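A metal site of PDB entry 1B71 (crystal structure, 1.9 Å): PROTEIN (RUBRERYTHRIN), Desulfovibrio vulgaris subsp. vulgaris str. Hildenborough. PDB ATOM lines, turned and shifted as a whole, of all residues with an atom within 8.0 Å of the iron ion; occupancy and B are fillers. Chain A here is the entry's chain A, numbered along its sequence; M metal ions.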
ATOM      1  N   ARG A 157      10.457   9.597 -28.025  1.00  0.00           N
ATOM      2  CA  ARG A 157      10.830  10.892 -27.464  1.00  0.00           C
ATOM      3  C   ARG A 157      10.158  11.087 -26.098  1.00  0.00           C
ATOM      4  O   ARG A 157       8.976  10.809 -25.920  1.00  0.00           O
ATOM      5  CB  ARG A 157      10.475  12.021 -28.437  1.00  0.00           C
ATOM      6  CG  ARG A 157      11.154  13.351 -28.119  1.00  0.00           C
ATOM      7  CD  ARG A 157      10.489  14.476 -28.876  1.00  0.00           C
ATOM      8  NE  ARG A 157       9.055  14.553 -28.578  1.00  0.00           N
ATOM      9  CZ  ARG A 157       8.444  15.714 -28.338  1.00  0.00           C
ATOM     10  NH1 ARG A 157       9.161  16.833 -28.367  1.00  0.00           N
ATOM     11  NH2 ARG A 157       7.142  15.778 -28.063  1.00  0.00           N
ATOM     12  N   CYS A 158      10.972  11.560 -25.165  1.00  0.00           N
ATOM     13  CA  CYS A 158      10.524  12.063 -23.878  1.00  0.00           C
ATOM     14  C   CYS A 158       9.746  13.368 -24.062  1.00  0.00           C
ATOM     15  O   CYS A 158      10.245  14.390 -24.526  1.00  0.00           O
ATOM     16  CB  CYS A 158      11.698  12.299 -22.925  1.00  0.00           C
ATOM     17  SG  CYS A 158      11.157  12.914 -21.320  1.00  0.00           S
ATOM     18  N   ARG A 159       8.470  13.313 -23.683  1.00  0.00           N
ATOM     19  CA  ARG A 159       7.650  14.512 -23.890  1.00  0.00           C
ATOM     20  C   ARG A 159       8.029  15.590 -22.888  1.00  0.00           C
ATOM     21  O   ARG A 159       7.828  16.781 -23.115  1.00  0.00           O
ATOM     22  CB  ARG A 159       6.175  14.127 -23.805  1.00  0.00           C
ATOM     23  CG  ARG A 159       5.830  13.054 -24.839  1.00  0.00           C
ATOM     24  CD  ARG A 159       4.335  12.969 -25.095  1.00  0.00           C
ATOM     25  NE  ARG A 159       3.875  14.175 -25.821  1.00  0.00           N
ATOM     26  CZ  ARG A 159       2.933  14.879 -25.194  1.00  0.00           C
ATOM     27  NH1 ARG A 159       2.548  14.381 -24.024  1.00  0.00           N
ATOM     28  NH2 ARG A 159       2.419  15.979 -25.709  1.00  0.00           N
ATOM     29  N   ASN A 160       8.577  15.132 -21.763  1.00  0.00           N
ATOM     30  CA  ASN A 160       8.957  16.058 -20.705  1.00  0.00           C
ATOM     31  C   ASN A 160      10.226  16.840 -21.020  1.00  0.00           C
ATOM     32  O   ASN A 160      10.294  18.037 -20.710  1.00  0.00           O
ATOM     33  CB  ASN A 160       9.115  15.302 -19.369  1.00  0.00           C
ATOM     34  CG  ASN A 160       9.366  16.292 -18.246  1.00  0.00           C
ATOM     35  OD1 ASN A 160       8.617  17.270 -18.105  1.00  0.00           O
ATOM     36  ND2 ASN A 160      10.421  16.034 -17.481  1.00  0.00           N
ATOM     37  N   CYS A 161      11.236  16.236 -21.650  1.00  0.00           N
ATOM     38  CA  CYS A 161      12.451  17.010 -21.857  1.00  0.00           C
ATOM     39  C   CYS A 161      13.041  16.861 -23.247  1.00  0.00           C
ATOM     40  O   CYS A 161      14.079  17.505 -23.437  1.00  0.00           O
ATOM     41  CB  CYS A 161      13.541  16.583 -20.878  1.00  0.00           C
ATOM     42  SG  CYS A 161      14.329  15.010 -21.337  1.00  0.00           S
ATOM     43  N   GLY A 162      12.443  16.099 -24.153  1.00  0.00           N
ATOM     44  CA  GLY A 162      12.884  16.042 -25.536  1.00  0.00           C
ATOM     45  C   GLY A 162      13.947  15.005 -25.814  1.00  0.00           C
ATOM     46  O   GLY A 162      14.483  14.840 -26.919  1.00  0.00           O
ATOM     47  N   TYR A 163      14.296  14.263 -24.756  1.00  0.00           N
ATOM     48  CA  TYR A 163      15.373  13.299 -24.888  1.00  0.00           C
ATOM     49  C   TYR A 163      14.956  12.258 -25.920  1.00  0.00           C
ATOM     50  O   TYR A 163      13.818  11.787 -25.850  1.00  0.00           O
ATOM     51  CB  TYR A 163      15.675  12.625 -23.542  1.00  0.00           C
ATOM     52  CG  TYR A 163      16.635  11.458 -23.738  1.00  0.00           C
ATOM     53  CD1 TYR A 163      17.991  11.711 -23.929  1.00  0.00           C
ATOM     54  CD2 TYR A 163      16.200  10.145 -23.735  1.00  0.00           C
ATOM     55  CE1 TYR A 163      18.892  10.689 -24.116  1.00  0.00           C
ATOM     56  CE2 TYR A 163      17.105   9.110 -23.923  1.00  0.00           C
ATOM     57  CZ  TYR A 163      18.442   9.393 -24.106  1.00  0.00           C
ATOM     58  OH  TYR A 163      19.331   8.375 -24.286  1.00  0.00           O
ATOM     59  N   VAL A 164      15.854  11.926 -26.847  1.00  0.00           N
ATOM     60  CA  VAL A 164      15.434  10.909 -27.819  1.00  0.00           C
ATOM     61  C   VAL A 164      16.169   9.599 -27.618  1.00  0.00           C
ATOM     62  O   VAL A 164      17.332   9.490 -27.240  1.00  0.00           O
ATOM     63  CB  VAL A 164      15.573  11.415 -29.265  1.00  0.00           C
ATOM     64  CG1 VAL A 164      15.147  10.346 -30.250  1.00  0.00           C
ATOM     65  CG2 VAL A 164      14.762  12.689 -29.449  1.00  0.00           C
ATOM     66  N   PRO A 171      12.263   3.939 -22.605  1.00  0.00           N
ATOM     67  CA  PRO A 171      13.008   3.563 -21.400  1.00  0.00           C
ATOM     68  C   PRO A 171      12.135   3.670 -20.151  1.00  0.00           C
ATOM     69  O   PRO A 171      11.145   4.404 -20.149  1.00  0.00           O
ATOM     70  CB  PRO A 171      14.128   4.606 -21.337  1.00  0.00           C
ATOM     71  CG  PRO A 171      13.519   5.816 -21.971  1.00  0.00           C
ATOM     72  CD  PRO A 171      12.601   5.298 -23.049  1.00  0.00           C
ATOM     73  N   LEU A 173      12.757   5.117 -17.558  1.00  0.00           N
ATOM     74  CA  LEU A 173      13.120   6.400 -16.978  1.00  0.00           C
ATOM     75  C   LEU A 173      13.936   7.198 -17.977  1.00  0.00           C
ATOM     76  O   LEU A 173      14.840   6.708 -18.655  1.00  0.00           O
ATOM     77  CB  LEU A 173      13.918   6.215 -15.682  1.00  0.00           C
ATOM     78  CG  LEU A 173      13.746   7.293 -14.603  1.00  0.00           C
ATOM     79  CD1 LEU A 173      12.631   6.947 -13.630  1.00  0.00           C
ATOM     80  CD2 LEU A 173      15.045   7.513 -13.846  1.00  0.00           C
ATOM     81  N   CYS A 174      13.588   8.485 -18.067  1.00  0.00           N
ATOM     82  CA  CYS A 174      14.363   9.288 -19.004  1.00  0.00           C
ATOM     83  C   CYS A 174      15.764   9.544 -18.454  1.00  0.00           C
ATOM     84  O   CYS A 174      15.954  10.103 -17.378  1.00  0.00           O
ATOM     85  CB  CYS A 174      13.649  10.613 -19.315  1.00  0.00           C
ATOM     86  SG  CYS A 174      14.608  11.622 -20.461  1.00  0.00           S
ATOM     87  N   PRO A 175      16.758   9.124 -19.237  1.00  0.00           N
ATOM     88  CA  PRO A 175      18.148   9.400 -18.878  1.00  0.00           C
ATOM     89  C   PRO A 175      18.366  10.889 -18.685  1.00  0.00           C
ATOM     90  O   PRO A 175      19.246  11.266 -17.905  1.00  0.00           O
ATOM     91  CB  PRO A 175      18.946   8.918 -20.090  1.00  0.00           C
ATOM     92  CG  PRO A 175      18.047   7.981 -20.826  1.00  0.00           C
ATOM     93  CD  PRO A 175      16.634   8.363 -20.499  1.00  0.00           C
ATOM     94  N   ALA A 176      17.588  11.727 -19.371  1.00  0.00           N
ATOM     95  CA  ALA A 176      17.823  13.171 -19.295  1.00  0.00           C
ATOM     96  C   ALA A 176      17.085  13.804 -18.118  1.00  0.00           C
ATOM     97  O   ALA A 176      17.717  14.356 -17.217  1.00  0.00           O
ATOM     98  CB  ALA A 176      17.474  13.818 -20.635  1.00  0.00           C
ATOM     99  N   CYS A 177      15.755  13.741 -18.096  1.00  0.00           N
ATOM    100  CA  CYS A 177      14.975  14.403 -17.049  1.00  0.00           C
ATOM    101  C   CYS A 177      14.548  13.487 -15.929  1.00  0.00           C
ATOM    102  O   CYS A 177      13.956  13.931 -14.935  1.00  0.00           O
ATOM    103  CB  CYS A 177      13.743  15.053 -17.711  1.00  0.00           C
ATOM    104  SG  CYS A 177      12.484  13.847 -18.207  1.00  0.00           S
ATOM    105  N   ALA A 178      14.819  12.186 -16.013  1.00  0.00           N
ATOM    106  CA  ALA A 178      14.486  11.255 -14.942  1.00  0.00           C
ATOM    107  C   ALA A 178      12.987  11.102 -14.733  1.00  0.00           C
ATOM    108  O   ALA A 178      12.518  10.565 -13.719  1.00  0.00           O
ATOM    109  CB  ALA A 178      15.165  11.698 -13.647  1.00  0.00           C
ATOM    110  N   HIS A 179      12.173  11.534 -15.689  1.00  0.00           N
ATOM    111  CA  HIS A 179      10.753  11.212 -15.662  1.00  0.00           C
ATOM    112  C   HIS A 179      10.509   9.802 -16.193  1.00  0.00           C
ATOM    113  O   HIS A 179      11.288   9.235 -16.958  1.00  0.00           O
ATOM    114  CB  HIS A 179       9.987  12.269 -16.466  1.00  0.00           C
ATOM    115  CG  HIS A 179       9.779  13.514 -15.666  1.00  0.00           C
ATOM    116  ND1 HIS A 179      10.834  14.255 -15.171  1.00  0.00           N
ATOM    117  CD2 HIS A 179       8.658  14.145 -15.267  1.00  0.00           C
ATOM    118  CE1 HIS A 179      10.361  15.301 -14.499  1.00  0.00           C
ATOM    119  NE2 HIS A 179       9.048  15.248 -14.546  1.00  0.00           N
ATOM    120  N   PRO A 180       9.396   9.180 -15.794  1.00  0.00           N
ATOM    121  CA  PRO A 180       9.113   7.790 -16.155  1.00  0.00           C
ATOM    122  C   PRO A 180       8.608   7.586 -17.570  1.00  0.00           C
ATOM    123  O   PRO A 180       8.251   8.511 -18.301  1.00  0.00           O
ATOM    124  CB  PRO A 180       7.998   7.399 -15.174  1.00  0.00           C
ATOM    125  CG  PRO A 180       7.388   8.672 -14.692  1.00  0.00           C
ATOM    126  CD  PRO A 180       8.356   9.789 -14.953  1.00  0.00           C
ATOM    127  N   HIS A 183       6.032   9.333 -19.995  1.00  0.00           N
ATOM    128  CA  HIS A 183       6.219  10.561 -20.771  1.00  0.00           C
ATOM    129  C   HIS A 183       6.735  10.306 -22.181  1.00  0.00           C
ATOM    130  O   HIS A 183       6.856  11.260 -22.958  1.00  0.00           O
ATOM    131  CB  HIS A 183       7.190  11.503 -20.041  1.00  0.00           C
ATOM    132  CG  HIS A 183       6.642  11.880 -18.700  1.00  0.00           C
ATOM    133  ND1 HIS A 183       6.132  13.125 -18.440  1.00  0.00           N
ATOM    134  CD2 HIS A 183       6.537  11.158 -17.559  1.00  0.00           C
ATOM    135  CE1 HIS A 183       5.731  13.165 -17.176  1.00  0.00           C
ATOM    136  NE2 HIS A 183       5.958  11.984 -16.616  1.00  0.00           N
ATOM    137  N   PHE A 184       7.034   9.061 -22.500  1.00  0.00           N
ATOM    138  CA  PHE A 184       7.576   8.747 -23.828  1.00  0.00           C
ATOM    139  C   PHE A 184       6.515   8.491 -24.885  1.00  0.00           C
ATOM    140  O   PHE A 184       5.435   7.941 -24.640  1.00  0.00           O
ATOM    141  CB  PHE A 184       8.493   7.509 -23.728  1.00  0.00           C
ATOM    142  CG  PHE A 184       9.888   7.970 -23.292  1.00  0.00           C
ATOM    143  CD1 PHE A 184      10.231   7.962 -21.961  1.00  0.00           C
ATOM    144  CD2 PHE A 184      10.770   8.416 -24.264  1.00  0.00           C
ATOM    145  CE1 PHE A 184      11.492   8.407 -21.584  1.00  0.00           C
ATOM    146  CE2 PHE A 184      12.034   8.856 -23.895  1.00  0.00           C
ATOM    147  CZ  PHE A 184      12.365   8.843 -22.551  1.00  0.00           C
HETATM  148 FE    FE M   1      13.170  13.350 -20.334  1.00  0.00          FE
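The iron ion is bound by SG of Cys 174 (2.3 Å), SG of Cys 161 (2.3 Å), SG of Cys 158 (2.3 Å) and SG of Cys 177 (2.3 Å). The iron ion has four donor atoms within binding distance.
N of Cys 158 sits at hydrogen-bond distance from O of Tyr 163, at 2.9 Å. O of Cys 177 sits at hydrogen-bond distance from ND1 of His 179 (3.1 Å). SG of Cys 161 sits close to N of Tyr 163 (3.5 Å). The backbone NH (N) of Ala 176 sits close to the side-chain sulfur (SG) of Cys 174, at 3.2 Å. The backbone NH of Cys 174 lies within hydrogen-bond range of the backbone carbonyl oxygen of His 179 (2.7 Å). ND2 of Asn 160 lies close to SG of Cys 177. The side-chain sulfur (SG) of Cys 158 lies close to the backbone NH (N) of Asn 160 (3.4 Å).
Within 4 Å of the iron ion: Cys 158, Cys 161, Cys 174 and Cys 177. Along chain A the residues within 4 Å of the iron ion span positions 158 to 177.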
